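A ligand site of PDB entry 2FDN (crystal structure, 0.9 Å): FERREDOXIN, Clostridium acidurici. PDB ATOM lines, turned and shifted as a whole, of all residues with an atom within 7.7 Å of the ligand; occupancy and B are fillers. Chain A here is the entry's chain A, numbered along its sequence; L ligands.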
ATOM      1  N   VAL A   3      -2.280   3.585  15.309  1.00  0.00           N
ATOM      2  CA  VAL A   3      -1.154   3.126  16.109  1.00  0.00           C
ATOM      3  C   VAL A   3      -1.408   3.651  17.540  1.00  0.00           C
ATOM      4  O   VAL A   3      -1.908   4.771  17.711  1.00  0.00           O
ATOM      5  CB  VAL A   3       0.194   3.606  15.552  1.00  0.00           C
ATOM      6  CG1 VAL A   3       0.341   5.100  15.572  1.00  0.00           C
ATOM      7  CG2 VAL A   3       1.374   2.939  16.226  1.00  0.00           C
ATOM      8  N   ILE A   4      -1.061   2.858  18.530  1.00  0.00           N
ATOM      9  CA  ILE A   4      -1.257   3.256  19.935  1.00  0.00           C
ATOM     10  C   ILE A   4      -0.009   3.939  20.416  1.00  0.00           C
ATOM     11  O   ILE A   4       1.108   3.373  20.484  1.00  0.00           O
ATOM     12  CB  ILE A   4      -1.620   2.032  20.802  1.00  0.00           C
ATOM     13  CG1 ILE A   4      -2.998   1.493  20.404  1.00  0.00           C
ATOM     14  CG2 ILE A   4      -1.592   2.424  22.286  1.00  0.00           C
ATOM     15  CD1 ILE A   4      -3.454   0.204  21.042  1.00  0.00           C
ATOM     16  N   ASN A   5      -0.209   5.178  20.821  1.00  0.00           N
ATOM     17  CA  ASN A   5       0.886   6.022  21.297  1.00  0.00           C
ATOM     18  C   ASN A   5       1.239   5.691  22.745  1.00  0.00           C
ATOM     19  O   ASN A   5       0.445   5.045  23.487  1.00  0.00           O
ATOM     20  CB  ASN A   5       0.501   7.491  21.191  1.00  0.00           C
ATOM     21  CG  ASN A   5       0.475   8.059  19.773  1.00  0.00           C
ATOM     22  OD1 ASN A   5       1.116   7.533  18.876  1.00  0.00           O
ATOM     23  ND2 ASN A   5      -0.198   9.200  19.619  1.00  0.00           N
ATOM     24  N   GLU A   6       2.388   6.169  23.178  1.00  0.00           N
ATOM     25  CA  GLU A   6       2.934   5.922  24.521  1.00  0.00           C
ATOM     26  C   GLU A   6       2.104   6.531  25.626  1.00  0.00           C
ATOM     27  O   GLU A   6       2.264   6.100  26.766  1.00  0.00           O
ATOM     28  CB  GLU A   6       4.378   6.448  24.626  1.00  0.00           C
ATOM     29  CG  GLU A   6       4.487   7.988  24.485  1.00  0.00           C
ATOM     30  CD  GLU A   6       4.505   8.667  25.843  1.00  0.00           C
ATOM     31  OE1 GLU A   6       5.339   8.337  26.716  1.00  0.00           O
ATOM     32  OE2 GLU A   6       3.663   9.611  26.090  1.00  0.00           O
ATOM     33  N   ALA A   7       1.130   7.454  25.286  1.00  0.00           N
ATOM     34  CA  ALA A   7       0.191   7.837  26.324  1.00  0.00           C
ATOM     35  C   ALA A   7      -0.568   6.701  26.898  1.00  0.00           C
ATOM     36  O   ALA A   7      -1.130   6.776  28.033  1.00  0.00           O
ATOM     37  CB  ALA A   7      -0.764   8.878  25.803  1.00  0.00           C
ATOM     38  N   CYS A   8      -0.695   5.587  26.178  1.00  0.00           N
ATOM     39  CA  CYS A   8      -1.379   4.439  26.683  1.00  0.00           C
ATOM     40  C   CYS A   8      -0.957   4.103  28.091  1.00  0.00           C
ATOM     41  O   CYS A   8       0.235   3.976  28.416  1.00  0.00           O
ATOM     42  CB  CYS A   8      -1.052   3.252  25.738  1.00  0.00           C
ATOM     43  SG  CYS A   8      -1.828   1.665  26.212  1.00  0.00           S
ATOM     44  N   ILE A   9      -1.967   3.924  28.963  1.00  0.00           N
ATOM     45  CA  ILE A   9      -1.821   3.542  30.370  1.00  0.00           C
ATOM     46  C   ILE A   9      -2.080   2.081  30.632  1.00  0.00           C
ATOM     47  O   ILE A   9      -2.063   1.641  31.741  1.00  0.00           O
ATOM     48  CB  ILE A   9      -2.639   4.461  31.293  1.00  0.00           C
ATOM     49  CG1 ILE A   9      -4.142   4.234  31.045  1.00  0.00           C
ATOM     50  CG2 ILE A   9      -2.229   5.901  31.074  1.00  0.00           C
ATOM     51  CD1 ILE A   9      -5.072   5.212  31.823  1.00  0.00           C
ATOM     52  N   SER A  10      -2.323   1.308  29.527  1.00  0.00           N
ATOM     53  CA  SER A  10      -2.444  -0.125  29.601  1.00  0.00           C
ATOM     54  C   SER A  10      -3.594  -0.568  30.504  1.00  0.00           C
ATOM     55  O   SER A  10      -3.560  -1.604  31.164  1.00  0.00           O
ATOM     56  CB  SER A  10      -1.124  -0.805  30.035  1.00  0.00           C
ATOM     57  OG  SER A  10      -0.180  -0.644  29.011  1.00  0.00           O
ATOM     58  N   CYS A  11      -4.728   0.142  30.329  1.00  0.00           N
ATOM     59  CA  CYS A  11      -5.950  -0.141  31.043  1.00  0.00           C
ATOM     60  C   CYS A  11      -6.707  -1.381  30.459  1.00  0.00           C
ATOM     61  O   CYS A  11      -7.589  -1.984  31.108  1.00  0.00           O
ATOM     62  CB  CYS A  11      -6.864   1.063  31.036  1.00  0.00           C
ATOM     63  SG  CYS A  11      -7.697   1.462  29.454  1.00  0.00           S
ATOM     64  N   GLY A  12      -6.442  -1.669  29.196  1.00  0.00           N
ATOM     65  CA  GLY A  12      -7.093  -2.778  28.525  1.00  0.00           C
ATOM     66  C   GLY A  12      -8.428  -2.533  27.923  1.00  0.00           C
ATOM     67  O   GLY A  12      -8.984  -3.415  27.294  1.00  0.00           O
ATOM     68  N   ALA A  13      -9.038  -1.364  28.076  1.00  0.00           N
ATOM     69  CA  ALA A  13     -10.427  -1.168  27.732  1.00  0.00           C
ATOM     70  C   ALA A  13     -10.723  -1.359  26.254  1.00  0.00           C
ATOM     71  O   ALA A  13     -11.829  -1.746  25.854  1.00  0.00           O
ATOM     72  CB  ALA A  13     -10.911   0.200  28.170  1.00  0.00           C
ATOM     73  N   CYS A  14      -9.740  -0.997  25.387  1.00  0.00           N
ATOM     74  CA  CYS A  14      -9.945  -1.039  23.944  1.00  0.00           C
ATOM     75  C   CYS A  14      -9.912  -2.432  23.410  1.00  0.00           C
ATOM     76  O   CYS A  14     -10.496  -2.672  22.289  1.00  0.00           O
ATOM     77  CB  CYS A  14      -8.864  -0.213  23.224  1.00  0.00           C
ATOM     78  SG  CYS A  14      -7.171  -0.732  23.680  1.00  0.00           S
ATOM     79  N   GLU A  15      -9.266  -3.387  24.014  1.00  0.00           N
ATOM     80  CA  GLU A  15      -9.037  -4.676  23.400  1.00  0.00           C
ATOM     81  C   GLU A  15     -10.306  -5.370  23.011  1.00  0.00           C
ATOM     82  O   GLU A  15     -10.425  -5.864  21.869  1.00  0.00           O
ATOM     83  CB  GLU A  15      -8.090  -5.514  24.238  1.00  0.00           C
ATOM     84  CG  GLU A  15      -7.784  -6.867  23.682  1.00  0.00           C
ATOM     85  CD  GLU A  15      -6.762  -7.672  24.418  1.00  0.00           C
ATOM     86  OE1 GLU A  15      -6.301  -7.262  25.455  1.00  0.00           O
ATOM     87  OE2 GLU A  15      -6.479  -8.833  24.086  1.00  0.00           O
ATOM     88  N   ILE A  23      -6.178  -5.636  18.448  1.00  0.00           N
ATOM     89  CA  ILE A  23      -5.394  -5.111  19.591  1.00  0.00           C
ATOM     90  C   ILE A  23      -4.992  -6.241  20.504  1.00  0.00           C
ATOM     91  O   ILE A  23      -5.779  -7.138  20.852  1.00  0.00           O
ATOM     92  CB  ILE A  23      -6.227  -4.033  20.356  1.00  0.00           C
ATOM     93  CG1 ILE A  23      -6.466  -2.872  19.418  1.00  0.00           C
ATOM     94  CG2 ILE A  23      -5.607  -3.670  21.660  1.00  0.00           C
ATOM     95  CD1 ILE A  23      -7.380  -1.795  19.956  1.00  0.00           C
ATOM     96  N   SER A  24      -3.753  -6.138  20.998  1.00  0.00           N
ATOM     97  CA  SER A  24      -3.258  -7.057  22.039  1.00  0.00           C
ATOM     98  C   SER A  24      -2.389  -6.236  22.984  1.00  0.00           C
ATOM     99  O   SER A  24      -1.991  -5.107  22.751  1.00  0.00           O
ATOM    100  CB  SER A  24      -2.472  -8.205  21.433  1.00  0.00           C
ATOM    101  OG  SER A  24      -1.365  -7.738  20.681  1.00  0.00           O
ATOM    102  N   SER A  25      -2.293  -6.912  24.233  1.00  0.00           N
ATOM    103  CA  SER A  25      -1.301  -6.263  25.083  1.00  0.00           C
ATOM    104  C   SER A  25       0.113  -6.562  24.570  1.00  0.00           C
ATOM    105  O   SER A  25       0.465  -7.744  24.498  1.00  0.00           O
ATOM    106  CB  SER A  25      -1.478  -6.700  26.530  1.00  0.00           C
ATOM    107  OG  SER A  25      -0.983  -8.032  26.590  1.00  0.00           O
ATOM    108  N   ARG A  29       3.091  -1.724  25.871  1.00  0.00           N
ATOM    109  CA  ARG A  29       1.767  -1.107  25.909  1.00  0.00           C
ATOM    110  C   ARG A  29       0.894  -1.892  24.925  1.00  0.00           C
ATOM    111  O   ARG A  29       1.331  -2.881  24.311  1.00  0.00           O
ATOM    112  CB  ARG A  29       1.837   0.348  25.511  1.00  0.00           C
ATOM    113  CG  ARG A  29       2.440   0.634  24.115  1.00  0.00           C
ATOM    114  CD  ARG A  29       2.564   2.115  23.834  1.00  0.00           C
ATOM    115  NE  ARG A  29       3.311   2.573  22.693  1.00  0.00           N
ATOM    116  CZ  ARG A  29       4.635   2.563  22.417  1.00  0.00           C
ATOM    117  NH1 ARG A  29       5.529   2.023  23.228  1.00  0.00           N
ATOM    118  NH2 ARG A  29       5.016   3.151  21.279  1.00  0.00           N
ATOM    119  N   TYR A  30      -0.288  -1.211  24.783  1.00  0.00           N
ATOM    120  CA  TYR A  30      -1.073  -2.054  23.890  1.00  0.00           C
ATOM    121  C   TYR A  30      -0.621  -1.776  22.450  1.00  0.00           C
ATOM    122  O   TYR A  30      -0.053  -0.720  22.160  1.00  0.00           O
ATOM    123  CB  TYR A  30      -2.543  -1.813  24.176  1.00  0.00           C
ATOM    124  CG  TYR A  30      -3.052  -2.658  25.328  1.00  0.00           C
ATOM    125  CD1 TYR A  30      -2.539  -2.543  26.605  1.00  0.00           C
ATOM    126  CD2 TYR A  30      -4.070  -3.551  25.140  1.00  0.00           C
ATOM    127  CE1 TYR A  30      -3.022  -3.314  27.656  1.00  0.00           C
ATOM    128  CE2 TYR A  30      -4.545  -4.349  26.184  1.00  0.00           C
ATOM    129  CZ  TYR A  30      -3.982  -4.234  27.428  1.00  0.00           C
ATOM    130  OH  TYR A  30      -4.480  -5.060  28.436  1.00  0.00           O
ATOM    131  N   VAL A  31      -0.930  -2.711  21.541  1.00  0.00           N
ATOM    132  CA  VAL A  31      -0.407  -2.624  20.161  1.00  0.00           C
ATOM    133  C   VAL A  31      -1.468  -3.136  19.180  1.00  0.00           C
ATOM    134  O   VAL A  31      -2.203  -4.072  19.407  1.00  0.00           O
ATOM    135  CB  VAL A  31       0.932  -3.374  20.050  1.00  0.00           C
ATOM    136  CG1 VAL A  31       0.757  -4.888  20.220  1.00  0.00           C
ATOM    137  CG2 VAL A  31       1.651  -3.039  18.756  1.00  0.00           C
ATOM    138  N   ILE A  32      -1.472  -2.427  18.050  1.00  0.00           N
ATOM    139  CA  ILE A  32      -2.379  -2.678  16.935  1.00  0.00           C
ATOM    140  C   ILE A  32      -1.686  -3.474  15.851  1.00  0.00           C
ATOM    141  O   ILE A  32      -0.551  -3.185  15.418  1.00  0.00           O
ATOM    142  CB  ILE A  32      -2.933  -1.355  16.359  1.00  0.00           C
ATOM    143  CG1 ILE A  32      -3.871  -0.738  17.410  1.00  0.00           C
ATOM    144  CG2 ILE A  32      -3.627  -1.561  15.006  1.00  0.00           C
ATOM    145  CD1 ILE A  32      -4.329   0.673  17.070  1.00  0.00           C
ATOM    146  N   ALA A  42     -12.662   2.939  16.907  1.00  0.00           N
ATOM    147  CA  ALA A  42     -13.383   2.571  18.143  1.00  0.00           C
ATOM    148  C   ALA A  42     -12.478   2.515  19.348  1.00  0.00           C
ATOM    149  O   ALA A  42     -12.919   2.833  20.458  1.00  0.00           O
ATOM    150  CB  ALA A  42     -14.084   1.229  17.973  1.00  0.00           C
ATOM    151  N   CYS A  43     -11.227   2.099  19.176  1.00  0.00           N
ATOM    152  CA  CYS A  43     -10.275   2.041  20.255  1.00  0.00           C
ATOM    153  C   CYS A  43     -10.027   3.428  20.863  1.00  0.00           C
ATOM    154  O   CYS A  43     -10.024   3.573  22.068  1.00  0.00           O
ATOM    155  CB  CYS A  43      -8.995   1.342  19.791  1.00  0.00           C
ATOM    156  SG  CYS A  43      -8.277   2.051  18.247  1.00  0.00           S
ATOM    157  N   ALA A  44      -9.808   4.424  20.004  1.00  0.00           N
ATOM    158  CA  ALA A  44      -9.647   5.771  20.500  1.00  0.00           C
ATOM    159  C   ALA A  44     -10.929   6.222  21.216  1.00  0.00           C
ATOM    160  O   ALA A  44     -10.863   6.896  22.252  1.00  0.00           O
ATOM    161  CB  ALA A  44      -9.267   6.733  19.378  1.00  0.00           C
ATOM    162  N   GLY A  45     -12.082   5.809  20.710  1.00  0.00           N
ATOM    163  CA  GLY A  45     -13.348   6.215  21.287  1.00  0.00           C
ATOM    164  C   GLY A  45     -13.567   5.672  22.701  1.00  0.00           C
ATOM    165  O   GLY A  45     -14.430   6.263  23.417  1.00  0.00           O
ATOM    166  N   VAL A  46     -12.911   4.602  23.100  1.00  0.00           N
ATOM    167  CA  VAL A  46     -13.007   4.062  24.447  1.00  0.00           C
ATOM    168  C   VAL A  46     -11.734   4.285  25.227  1.00  0.00           C
ATOM    169  O   VAL A  46     -11.531   3.714  26.319  1.00  0.00           O
ATOM    170  CB  VAL A  46     -13.458   2.619  24.497  1.00  0.00           C
ATOM    171  CG1 VAL A  46     -14.837   2.497  23.850  1.00  0.00           C
ATOM    172  CG2 VAL A  46     -12.458   1.666  23.861  1.00  0.00           C
ATOM    173  N   CYS A  47     -10.801   5.139  24.736  1.00  0.00           N
ATOM    174  CA  CYS A  47      -9.525   5.324  25.343  1.00  0.00           C
ATOM    175  C   CYS A  47      -9.537   6.567  26.202  1.00  0.00           C
ATOM    176  O   CYS A  47      -9.644   7.692  25.635  1.00  0.00           O
ATOM    177  CB  CYS A  47      -8.408   5.417  24.303  1.00  0.00           C
ATOM    178  SG  CYS A  47      -6.815   5.620  25.199  1.00  0.00           S
ATOM    179  N   PRO A  48      -9.349   6.506  27.527  1.00  0.00           N
ATOM    180  CA  PRO A  48      -9.450   7.721  28.343  1.00  0.00           C
ATOM    181  C   PRO A  48      -8.388   8.734  28.050  1.00  0.00           C
ATOM    182  O   PRO A  48      -8.557   9.926  28.356  1.00  0.00           O
ATOM    183  CB  PRO A  48      -9.336   7.196  29.787  1.00  0.00           C
ATOM    184  CG  PRO A  48      -8.601   5.886  29.667  1.00  0.00           C
ATOM    185  CD  PRO A  48      -9.112   5.285  28.353  1.00  0.00           C
ATOM    186  N   VAL A  49      -7.245   8.297  27.504  1.00  0.00           N
ATOM    187  CA  VAL A  49      -6.104   9.162  27.231  1.00  0.00           C
ATOM    188  C   VAL A  49      -5.924   9.403  25.745  1.00  0.00           C
ATOM    189  O   VAL A  49      -4.903  10.007  25.353  1.00  0.00           O
ATOM    190  CB  VAL A  49      -4.835   8.611  27.881  1.00  0.00           C
ATOM    191  CG1 VAL A  49      -4.991   8.674  29.399  1.00  0.00           C
ATOM    192  CG2 VAL A  49      -4.455   7.230  27.342  1.00  0.00           C
ATOM    193  N   ASP A  50      -6.844   8.925  24.883  1.00  0.00           N
ATOM    194  CA  ASP A  50      -6.800   9.155  23.463  1.00  0.00           C
ATOM    195  C   ASP A  50      -5.456   8.745  22.824  1.00  0.00           C
ATOM    196  O   ASP A  50      -4.933   9.427  21.934  1.00  0.00           O
ATOM    197  CB  ASP A  50      -7.108  10.616  23.168  1.00  0.00           C
ATOM    198  CG  ASP A  50      -7.661  10.865  21.778  1.00  0.00           C
ATOM    199  OD1 ASP A  50      -8.469  10.011  21.278  1.00  0.00           O
ATOM    200  OD2 ASP A  50      -7.254  11.862  21.177  1.00  0.00           O
ATOM    201  N   ALA A  51      -4.973   7.567  23.212  1.00  0.00           N
ATOM    202  CA  ALA A  51      -3.664   7.110  22.715  1.00  0.00           C
ATOM    203  C   ALA A  51      -3.682   6.575  21.274  1.00  0.00           C
ATOM    204  O   ALA A  51      -2.663   6.757  20.575  1.00  0.00           O
ATOM    205  CB  ALA A  51      -3.124   6.024  23.655  1.00  0.00           C
ATOM    206  N   PRO A  52      -4.730   5.888  20.785  1.00  0.00           N
ATOM    207  CA  PRO A  52      -4.701   5.408  19.415  1.00  0.00           C
ATOM    208  C   PRO A  52      -4.956   6.555  18.454  1.00  0.00           C
ATOM    209  O   PRO A  52      -5.952   7.266  18.605  1.00  0.00           O
ATOM    210  CB  PRO A  52      -5.830   4.376  19.360  1.00  0.00           C
ATOM    211  CG  PRO A  52      -6.176   4.084  20.813  1.00  0.00           C
ATOM    212  CD  PRO A  52      -5.876   5.378  21.512  1.00  0.00           C
HETATM  213 FE1  LIG L   1      -4.075   1.920  26.102  1.00  0.00          FE
HETATM  214 FE2  LIG L   1      -6.364   1.706  27.637  1.00  0.00          FE
HETATM  215 FE3  LIG L   1      -6.314   0.865  24.981  1.00  0.00          FE
HETATM  216 FE4  LIG L   1      -6.214   3.482  25.591  1.00  0.00          FE
HETATM  217  S1  LIG L   1      -7.951   2.089  25.995  1.00  0.00           S
HETATM  218  S2  LIG L   1      -4.945   2.423  24.043  1.00  0.00           S
HETATM  219  S3  LIG L   1      -4.968   3.490  27.515  1.00  0.00           S
HETATM  220  S4  LIG L   1      -5.086   0.000  26.731  1.00  0.00           S
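The side-chain sulfur (SG) of Cys 47 lies close to the backbone NH (N) of Val 49 (3.6 Å). The side-chain sulfur (SG) of Cys 11 lies close to the backbone NH (N) of Ala 13, at 3.4 Å. NE of Arg 29 is in hydrogen-bond range of O of Ile 4 (3.2 Å). The backbone NH (N) of Ala 51 lies close to the side-chain sulfur (SG) of Cys 47 (3.3 Å). The side-chain sulfur (SG) of Cys 47 lies close to the backbone NH (N) of Asp 50, 3.3 Å away. The backbone NH (N) of Ser 10 lies close to the side-chain sulfur (SG) of Cys 8 (3.4 Å). The backbone NH (N) of Tyr 30 sits close to the side-chain sulfur (SG) of Cys 8 (3.6 Å).
The side-chain sulfur of Cys 8 binds an iron atom (FE1) of the ligand (2.3 Å). An iron atom (FE4) of the ligand is bound by the side-chain sulfur (SG) of Cys 47 (2.3 Å). The backbone NH of Ile 9 sits close to a sulfur (S3) of the ligand. S1 of the ligand lies close to N of Cys 14, 3.6 Å away. The backbone NH (N) of Gly 12 lies close to a sulfur (S4) of the ligand (3.3 Å). N of Cys 11 sits close to S4 of the ligand, 3.6 Å away. The side-chain sulfur of Cys 11 binds an iron atom (FE2) of the ligand (2.3 Å). The side-chain sulfur (SG) of Cys 14 is bound to an iron atom (FE3) of the ligand (2.2 Å).
Ile 4 touches the ligand (CG2 to S2, 3.8 Å). N of Ser 10 touches FE1 of the ligand, at 3.9 Å. Tyr 30 touches the ligand (CD1 to S4, 3.6 Å). Val 46 touches the ligand (O to S1, 3.9 Å). Val 49 touches the ligand (CG2 to S3, 3.8 Å). Pro 52 touches the ligand (CG to S2, 3.8 Å). 12 residues have an atom within 4 Å of the ligand: Ile 4, Cys 8, Ile 9, Ser 10, Cys 11, Gly 12, Cys 14, Tyr 30, Val 46, Cys 47, Val 49 and Pro 52. The nearest printed residue that does not touch the ligand is Ala 51 (4.1 Å).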
